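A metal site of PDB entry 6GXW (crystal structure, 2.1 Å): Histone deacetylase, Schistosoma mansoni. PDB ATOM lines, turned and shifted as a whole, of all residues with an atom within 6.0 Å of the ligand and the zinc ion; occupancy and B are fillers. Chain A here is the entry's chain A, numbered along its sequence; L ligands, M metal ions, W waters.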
ATOM      1  N   LYS A  21       2.168   6.121  -1.344  1.00  0.00           N
ATOM      2  CA  LYS A  21       1.186   6.398  -2.396  1.00  0.00           C
ATOM      3  C   LYS A  21       1.556   7.628  -3.231  1.00  0.00           C
ATOM      4  O   LYS A  21       1.478   7.589  -4.457  1.00  0.00           O
ATOM      5  CB  LYS A  21      -0.201   6.584  -1.787  1.00  0.00           C
ATOM      6  CG  LYS A  21      -1.217   7.060  -2.814  1.00  0.00           C
ATOM      7  CD  LYS A  21      -2.522   7.452  -2.202  1.00  0.00           C
ATOM      8  CE  LYS A  21      -3.646   7.186  -3.179  1.00  0.00           C
ATOM      9  NZ  LYS A  21      -3.587   5.769  -3.622  1.00  0.00           N
ATOM     10  N   PHE A  22       1.936   8.736  -2.585  1.00  0.00           N
ATOM     11  CA  PHE A  22       2.169   9.962  -3.326  1.00  0.00           C
ATOM     12  C   PHE A  22       3.634  10.204  -3.631  1.00  0.00           C
ATOM     13  O   PHE A  22       3.953  11.223  -4.241  1.00  0.00           O
ATOM     14  CB  PHE A  22       1.580  11.168  -2.562  1.00  0.00           C
ATOM     15  CG  PHE A  22       0.077  11.206  -2.581  1.00  0.00           C
ATOM     16  CD1 PHE A  22      -0.598  11.652  -3.713  1.00  0.00           C
ATOM     17  CD2 PHE A  22      -0.661  10.785  -1.483  1.00  0.00           C
ATOM     18  CE1 PHE A  22      -1.991  11.681  -3.740  1.00  0.00           C
ATOM     19  CE2 PHE A  22      -2.047  10.806  -1.510  1.00  0.00           C
ATOM     20  CZ  PHE A  22      -2.713  11.261  -2.648  1.00  0.00           C
ATOM     21  N   ASP A 101      -6.520   0.856   2.298  1.00  0.00           N
ATOM     22  CA  ASP A 101      -6.227   2.096   1.585  1.00  0.00           C
ATOM     23  C   ASP A 101      -5.468   3.124   2.427  1.00  0.00           C
ATOM     24  O   ASP A 101      -4.942   4.086   1.875  1.00  0.00           O
ATOM     25  CB  ASP A 101      -7.540   2.714   1.046  1.00  0.00           C
ATOM     26  CG  ASP A 101      -8.601   2.942   2.142  1.00  0.00           C
ATOM     27  OD1 ASP A 101      -8.593   2.222   3.170  1.00  0.00           O
ATOM     28  OD2 ASP A 101      -9.451   3.862   1.960  1.00  0.00           O
ATOM     29  N   HIS A 142      -8.965  15.707   2.563  1.00  0.00           N
ATOM     30  CA  HIS A 142     -10.333  16.007   2.928  1.00  0.00           C
ATOM     31  C   HIS A 142     -11.160  14.791   3.364  1.00  0.00           C
ATOM     32  O   HIS A 142     -12.299  14.987   3.770  1.00  0.00           O
ATOM     33  CB  HIS A 142     -11.036  16.710   1.754  1.00  0.00           C
ATOM     34  CG  HIS A 142     -11.015  15.944   0.460  1.00  0.00           C
ATOM     35  ND1 HIS A 142     -11.716  16.366  -0.662  1.00  0.00           N
ATOM     36  CD2 HIS A 142     -10.366  14.812   0.084  1.00  0.00           C
ATOM     37  CE1 HIS A 142     -11.508  15.521  -1.645  1.00  0.00           C
ATOM     38  NE2 HIS A 142     -10.690  14.569  -1.226  1.00  0.00           N
ATOM     39  N   HIS A 143     -10.660  13.563   3.267  1.00  0.00           N
ATOM     40  CA  HIS A 143     -11.471  12.415   3.658  1.00  0.00           C
ATOM     41  C   HIS A 143     -11.291  12.004   5.112  1.00  0.00           C
ATOM     42  O   HIS A 143     -12.089  11.203   5.605  1.00  0.00           O
ATOM     43  CB  HIS A 143     -11.167  11.184   2.789  1.00  0.00           C
ATOM     44  CG  HIS A 143     -11.396  11.403   1.322  1.00  0.00           C
ATOM     45  ND1 HIS A 143     -12.618  11.754   0.798  1.00  0.00           N
ATOM     46  CD2 HIS A 143     -10.552  11.289   0.265  1.00  0.00           C
ATOM     47  CE1 HIS A 143     -12.521  11.847  -0.516  1.00  0.00           C
ATOM     48  NE2 HIS A 143     -11.285  11.576  -0.864  1.00  0.00           N
ATOM     49  N   GLY A 151      -9.287   6.994   2.433  1.00  0.00           N
ATOM     50  CA  GLY A 151      -8.809   7.481   1.151  1.00  0.00           C
ATOM     51  C   GLY A 151      -7.406   8.091   1.209  1.00  0.00           C
ATOM     52  O   GLY A 151      -7.157   9.154   0.635  1.00  0.00           O
ATOM     53  N   PHE A 152      -6.513   7.403   1.917  1.00  0.00           N
ATOM     54  CA  PHE A 152      -5.152   7.852   2.203  1.00  0.00           C
ATOM     55  C   PHE A 152      -5.106   9.211   2.910  1.00  0.00           C
ATOM     56  O   PHE A 152      -4.081   9.901   2.865  1.00  0.00           O
ATOM     57  CB  PHE A 152      -4.269   7.869   0.952  1.00  0.00           C
ATOM     58  CG  PHE A 152      -2.836   7.536   1.247  1.00  0.00           C
ATOM     59  CD1 PHE A 152      -2.454   6.224   1.461  1.00  0.00           C
ATOM     60  CD2 PHE A 152      -1.871   8.546   1.366  1.00  0.00           C
ATOM     61  CE1 PHE A 152      -1.144   5.902   1.760  1.00  0.00           C
ATOM     62  CE2 PHE A 152      -0.554   8.229   1.668  1.00  0.00           C
ATOM     63  CZ  PHE A 152      -0.191   6.901   1.863  1.00  0.00           C
ATOM     64  N   CYS A 153      -6.190   9.599   3.604  1.00  0.00           N
ATOM     65  CA  CYS A 153      -6.211  10.802   4.429  1.00  0.00           C
ATOM     66  C   CYS A 153      -6.222  10.382   5.888  1.00  0.00           C
ATOM     67  O   CYS A 153      -7.195   9.786   6.366  1.00  0.00           O
ATOM     68  CB  CYS A 153      -7.425  11.667   4.096  1.00  0.00           C
ATOM     69  SG  CYS A 153      -7.464  12.235   2.353  1.00  0.00           S
ATOM     70  N   ASP A 187     -11.732  18.714  -6.047  1.00  0.00           N
ATOM     71  CA  ASP A 187     -11.281  17.350  -6.270  1.00  0.00           C
ATOM     72  C   ASP A 187     -12.350  16.526  -7.013  1.00  0.00           C
ATOM     73  O   ASP A 187     -13.551  16.764  -6.874  1.00  0.00           O
ATOM     74  CB  ASP A 187     -10.966  16.739  -4.913  1.00  0.00           C
ATOM     75  CG  ASP A 187     -10.123  15.508  -4.982  1.00  0.00           C
ATOM     76  OD1 ASP A 187     -10.675  14.415  -5.265  1.00  0.00           O
ATOM     77  OD2 ASP A 187      -8.901  15.605  -4.725  1.00  0.00           O
ATOM     78  N   LEU A 188     -11.892  15.565  -7.817  1.00  0.00           N
ATOM     79  CA  LEU A 188     -12.800  14.588  -8.420  1.00  0.00           C
ATOM     80  C   LEU A 188     -13.725  13.919  -7.390  1.00  0.00           C
ATOM     81  O   LEU A 188     -14.872  13.581  -7.716  1.00  0.00           O
ATOM     82  CB  LEU A 188     -11.988  13.527  -9.152  1.00  0.00           C
ATOM     83  CG  LEU A 188     -12.775  12.403  -9.833  1.00  0.00           C
ATOM     84  CD1 LEU A 188     -13.683  12.976 -10.886  1.00  0.00           C
ATOM     85  CD2 LEU A 188     -11.865  11.361 -10.443  1.00  0.00           C
ATOM     86  N   HIS A 189     -13.268  13.705  -6.163  1.00  0.00           N
ATOM     87  CA  HIS A 189     -14.015  12.941  -5.186  1.00  0.00           C
ATOM     88  C   HIS A 189     -14.706  13.851  -4.165  1.00  0.00           C
ATOM     89  O   HIS A 189     -14.239  14.949  -3.860  1.00  0.00           O
ATOM     90  CB  HIS A 189     -13.096  11.968  -4.442  1.00  0.00           C
ATOM     91  CG  HIS A 189     -12.344  11.044  -5.347  1.00  0.00           C
ATOM     92  ND1 HIS A 189     -11.064  11.297  -5.766  1.00  0.00           N
ATOM     93  CD2 HIS A 189     -12.693   9.854  -5.898  1.00  0.00           C
ATOM     94  CE1 HIS A 189     -10.650  10.310  -6.544  1.00  0.00           C
ATOM     95  NE2 HIS A 189     -11.618   9.419  -6.637  1.00  0.00           N
ATOM     96  N   HIS A 190     -15.834  13.357  -3.638  1.00  0.00           N
ATOM     97  CA  HIS A 190     -16.589  14.144  -2.671  1.00  0.00           C
ATOM     98  C   HIS A 190     -15.762  14.449  -1.418  1.00  0.00           C
ATOM     99  O   HIS A 190     -15.145  13.557  -0.822  1.00  0.00           O
ATOM    100  CB  HIS A 190     -17.869  13.396  -2.279  1.00  0.00           C
ATOM    101  CG  HIS A 190     -18.664  14.091  -1.226  1.00  0.00           C
ATOM    102  ND1 HIS A 190     -18.974  13.500  -0.023  1.00  0.00           N
ATOM    103  CD2 HIS A 190     -19.173  15.338  -1.180  1.00  0.00           C
ATOM    104  CE1 HIS A 190     -19.686  14.355   0.707  1.00  0.00           C
ATOM    105  NE2 HIS A 190     -19.809  15.477   0.027  1.00  0.00           N
ATOM    106  N   PHE A 217     -15.993   5.760  -4.866  1.00  0.00           N
ATOM    107  CA  PHE A 217     -15.524   6.362  -3.620  1.00  0.00           C
ATOM    108  C   PHE A 217     -15.840   7.849  -3.569  1.00  0.00           C
ATOM    109  O   PHE A 217     -15.663   8.533  -4.562  1.00  0.00           O
ATOM    110  CB  PHE A 217     -14.004   6.149  -3.478  1.00  0.00           C
ATOM    111  CG  PHE A 217     -13.451   6.625  -2.167  1.00  0.00           C
ATOM    112  CD1 PHE A 217     -13.548   5.823  -1.025  1.00  0.00           C
ATOM    113  CD2 PHE A 217     -12.835   7.872  -2.056  1.00  0.00           C
ATOM    114  CE1 PHE A 217     -13.061   6.254   0.208  1.00  0.00           C
ATOM    115  CE2 PHE A 217     -12.318   8.302  -0.827  1.00  0.00           C
ATOM    116  CZ  PHE A 217     -12.436   7.482   0.306  1.00  0.00           C
ATOM    117  N   GLN A 282      -9.964  23.510  -2.001  1.00  0.00           N
ATOM    118  CA  GLN A 282      -9.203  22.288  -2.224  1.00  0.00           C
ATOM    119  C   GLN A 282      -9.150  22.063  -3.724  1.00  0.00           C
ATOM    120  O   GLN A 282     -10.183  22.035  -4.395  1.00  0.00           O
ATOM    121  CB  GLN A 282      -9.807  21.106  -1.465  1.00  0.00           C
ATOM    122  CG  GLN A 282      -8.885  19.916  -1.317  1.00  0.00           C
ATOM    123  CD  GLN A 282      -9.179  18.850  -2.343  1.00  0.00           C
ATOM    124  OE1 GLN A 282      -9.833  19.125  -3.339  1.00  0.00           O
ATOM    125  NE2 GLN A 282      -8.713  17.639  -2.106  1.00  0.00           N
ATOM    126  N   GLY A 284      -7.809  19.482  -5.737  1.00  0.00           N
ATOM    127  CA  GLY A 284      -7.391  18.172  -6.187  1.00  0.00           C
ATOM    128  C   GLY A 284      -7.281  18.092  -7.694  1.00  0.00           C
ATOM    129  O   GLY A 284      -8.162  18.576  -8.403  1.00  0.00           O
ATOM    130  N   ASP A 286      -7.137  15.404  -9.614  1.00  0.00           N
ATOM    131  CA  ASP A 286      -7.521  14.158 -10.260  1.00  0.00           C
ATOM    132  C   ASP A 286      -8.676  14.334 -11.229  1.00  0.00           C
ATOM    133  O   ASP A 286      -9.061  13.355 -11.867  1.00  0.00           O
ATOM    134  CB  ASP A 286      -7.843  13.063  -9.226  1.00  0.00           C
ATOM    135  CG  ASP A 286      -8.498  13.612  -7.973  1.00  0.00           C
ATOM    136  OD1 ASP A 286      -8.981  14.763  -7.985  1.00  0.00           O
ATOM    137  OD2 ASP A 286      -8.515  12.871  -6.977  1.00  0.00           O
ATOM    138  N   ASP A 291      -5.338  12.019 -15.678  1.00  0.00           N
ATOM    139  CA  ASP A 291      -5.214  11.266 -14.430  1.00  0.00           C
ATOM    140  C   ASP A 291      -5.551   9.800 -14.672  1.00  0.00           C
ATOM    141  O   ASP A 291      -6.476   9.494 -15.444  1.00  0.00           O
ATOM    142  CB  ASP A 291      -6.169  11.845 -13.388  1.00  0.00           C
ATOM    143  CG  ASP A 291      -5.892  11.307 -11.993  1.00  0.00           C
ATOM    144  OD1 ASP A 291      -6.486  10.261 -11.633  1.00  0.00           O
ATOM    145  OD2 ASP A 291      -5.060  11.934 -11.276  1.00  0.00           O
ATOM    146  N   PRO A 292      -4.864   8.862 -14.017  1.00  0.00           N
ATOM    147  CA  PRO A 292      -5.215   7.437 -14.180  1.00  0.00           C
ATOM    148  C   PRO A 292      -6.648   7.102 -13.794  1.00  0.00           C
ATOM    149  O   PRO A 292      -7.129   6.019 -14.163  1.00  0.00           O
ATOM    150  CB  PRO A 292      -4.215   6.708 -13.278  1.00  0.00           C
ATOM    151  CG  PRO A 292      -3.113   7.650 -13.079  1.00  0.00           C
ATOM    152  CD  PRO A 292      -3.658   9.030 -13.190  1.00  0.00           C
ATOM    153  N   HIS A 293      -7.352   7.977 -13.058  1.00  0.00           N
ATOM    154  CA  HIS A 293      -8.793   7.825 -12.864  1.00  0.00           C
ATOM    155  C   HIS A 293      -9.543   7.926 -14.186  1.00  0.00           C
ATOM    156  O   HIS A 293     -10.378   7.077 -14.511  1.00  0.00           O
ATOM    157  CB  HIS A 293      -9.334   8.884 -11.911  1.00  0.00           C
ATOM    158  CG  HIS A 293      -9.398   8.443 -10.479  1.00  0.00           C
ATOM    159  ND1 HIS A 293      -8.328   8.583  -9.606  1.00  0.00           N
ATOM    160  CD2 HIS A 293     -10.399   7.885  -9.758  1.00  0.00           C
ATOM    161  CE1 HIS A 293      -8.675   8.119  -8.415  1.00  0.00           C
ATOM    162  NE2 HIS A 293      -9.916   7.694  -8.477  1.00  0.00           N
ATOM    163  N   GLY A 339      -4.335  18.093  -2.939  1.00  0.00           N
ATOM    164  CA  GLY A 339      -5.230  16.994  -2.714  1.00  0.00           C
ATOM    165  C   GLY A 339      -4.866  15.844  -3.625  1.00  0.00           C
ATOM    166  O   GLY A 339      -3.676  15.570  -3.827  1.00  0.00           O
ATOM    167  N   GLY A 340      -5.881  15.199  -4.178  1.00  0.00           N
ATOM    168  CA  GLY A 340      -5.665  14.105  -5.121  1.00  0.00           C
ATOM    169  C   GLY A 340      -4.929  14.594  -6.352  1.00  0.00           C
ATOM    170  O   GLY A 340      -4.725  15.786  -6.571  1.00  0.00           O
ATOM    171  N   GLY A 341      -4.514  13.649  -7.183  1.00  0.00           N
ATOM    172  CA  GLY A 341      -3.619  13.956  -8.281  1.00  0.00           C
ATOM    173  C   GLY A 341      -2.597  12.846  -8.427  1.00  0.00           C
ATOM    174  O   GLY A 341      -1.582  12.832  -7.728  1.00  0.00           O
ATOM    175  N   TYR A 342      -2.861  11.899  -9.345  1.00  0.00           N
ATOM    176  CA  TYR A 342      -2.099  10.649  -9.385  1.00  0.00           C
ATOM    177  C   TYR A 342      -1.192  10.553 -10.592  1.00  0.00           C
ATOM    178  O   TYR A 342      -0.335   9.657 -10.634  1.00  0.00           O
ATOM    179  CB  TYR A 342      -3.092   9.464  -9.308  1.00  0.00           C
ATOM    180  CG  TYR A 342      -3.846   9.616  -8.021  1.00  0.00           C
ATOM    181  CD1 TYR A 342      -3.217   9.329  -6.812  1.00  0.00           C
ATOM    182  CD2 TYR A 342      -5.114  10.185  -7.981  1.00  0.00           C
ATOM    183  CE1 TYR A 342      -3.846   9.540  -5.608  1.00  0.00           C
ATOM    184  CE2 TYR A 342      -5.758  10.409  -6.767  1.00  0.00           C
ATOM    185  CZ  TYR A 342      -5.115  10.081  -5.575  1.00  0.00           C
ATOM    186  OH  TYR A 342      -5.710  10.269  -4.337  1.00  0.00           O
HETATM  187  C1  LIG L   1      -8.781   9.179  -3.077  1.00  0.00           C
HETATM  188  C2  LIG L   1      -8.472   8.167  -3.885  1.00  0.00           C
HETATM  189  C3  LIG L   1      -8.896   6.765  -3.734  1.00  0.00           C
HETATM  190  C4  LIG L   1      -9.700   6.378  -2.653  1.00  0.00           C
HETATM  191  C5  LIG L   1     -10.138   5.072  -2.537  1.00  0.00           C
HETATM  192  C6  LIG L   1      -9.773   4.124  -3.475  1.00  0.00           C
HETATM  193  C7  LIG L   1      -8.973   4.481  -4.552  1.00  0.00           C
HETATM  194  C8  LIG L   1      -8.525   5.796  -4.675  1.00  0.00           C
HETATM  195  C9  LIG L   1      -7.539   5.342  -6.817  1.00  0.00           C
HETATM  196  O1  LIG L   1      -7.699   6.214  -5.680  1.00  0.00           O
HETATM  197  C10 LIG L   1      -6.066   5.268  -7.139  1.00  0.00           C
HETATM  198  C11 LIG L   1      -5.584   5.518  -8.431  1.00  0.00           C
HETATM  199  C12 LIG L   1      -4.249   5.389  -8.777  1.00  0.00           C
HETATM  200  C13 LIG L   1      -3.337   4.996  -7.809  1.00  0.00           C
HETATM  201  C14 LIG L   1      -3.761   4.745  -6.524  1.00  0.00           C
HETATM  202  C15 LIG L   1      -5.097   4.886  -6.197  1.00  0.00           C
HETATM  203  N1  LIG L   1      -9.074  11.474  -2.627  1.00  0.00           N
HETATM  204  C16 LIG L   1      -8.582  10.598  -3.488  1.00  0.00           C
HETATM  205  O2  LIG L   1      -8.060  10.920  -4.565  1.00  0.00           O
HETATM  206  O3  LIG L   1     -10.107  12.326  -3.026  1.00  0.00           O
HETATM  207 CL1  LIG L   1      -6.696   6.004  -9.677  1.00  0.00          CL
HETATM  208 CL2  LIG L   1      -5.559   4.597  -4.552  1.00  0.00          CL
HETATM  209 ZN    ZN M   1      -9.577  12.741  -5.310  1.00  0.00          ZN
HETATM  210  O   HOH W   1      -6.164  11.315  -1.041  1.00  0.00           O
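The side-chain hydroxyl (OH) of Tyr 342 lies close to an oxygen (O2) of the ligand (2.4 Å). A ring nitrogen (NE2) of His 142 lies close to an oxygen (O3) of the ligand (2.9 Å). NE2 of His 143 sits at hydrogen-bond distance from N1 of the ligand.
NE2 of His 189 is in hydrogen-bond range of NE2 of His 293 (3.0 Å). The side-chain sulfur (SG) of Cys 153 lies within hydrogen-bond range of the backbone NH (N) of His 142 (3.8 Å). OD2 of Asp 187 lies within hydrogen-bond range of N of Gly 340 (3.1 Å). A ring nitrogen (NE2) of His 142 lies within hydrogen-bond range of a ring nitrogen (NE2) of His 143 (3.1 Å). The backbone NH (N) of His 293 is in hydrogen-bond range of the side-chain carboxylate (OD1) of Asp 291, 2.8 Å away. OD2 of Asp 187 is in hydrogen-bond range of NE2 of Gln 282, 3.3 Å away. The side-chain carboxylate of Asp 291 sits at hydrogen-bond distance from the backbone NH of Tyr 342, at 2.9 Å. The side-chain sulfur (SG) of Cys 153 sits at hydrogen-bond distance from the backbone NH (N) of His 143, 3.6 Å away.
NZ of Lys 21 touches CL2 of the ligand, 2.5 Å away. Phe 217 touches the ligand. ND1 of His 293 touches CL1 of the ligand, at 3.1 Å. Hydrophobic or aromatic side chains that line the ligand: His 142, His 143, His 189, Phe 217, His 293 and Tyr 342. Within 4 Å of the ligand: Lys 21, His 142, His 143, Asp 187, His 189, Phe 217, Asp 286, His 293 and Tyr 342.
Of the 23 residues printed, 3 come within 4 Å of the zinc ion. The nearest printed residue that does not touch the zinc ion is Gly 340 (4.1 Å).
The zinc ion is bound by the side-chain carboxylate of Asp 286 (2.0 Å), the side-chain carboxylate of Asp 187 (2.0 Å), a ring nitrogen (ND1) of His 189 (2.1 Å), an oxygen (O3) of the ligand (2.4 Å) and an oxygen (O2) of the ligand (2.5 Å). The zinc ion has five donor atoms within binding distance.
Water W1 lies within hydrogen-bond range of the backbone carbonyl oxygen of Gly 151 (2.9 Å), a nitrogen (N1) of the ligand (3.3 Å), the side-chain hydroxyl of Tyr 342 (3.5 Å) and the side-chain sulfur of Cys 153 (3.7 Å).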
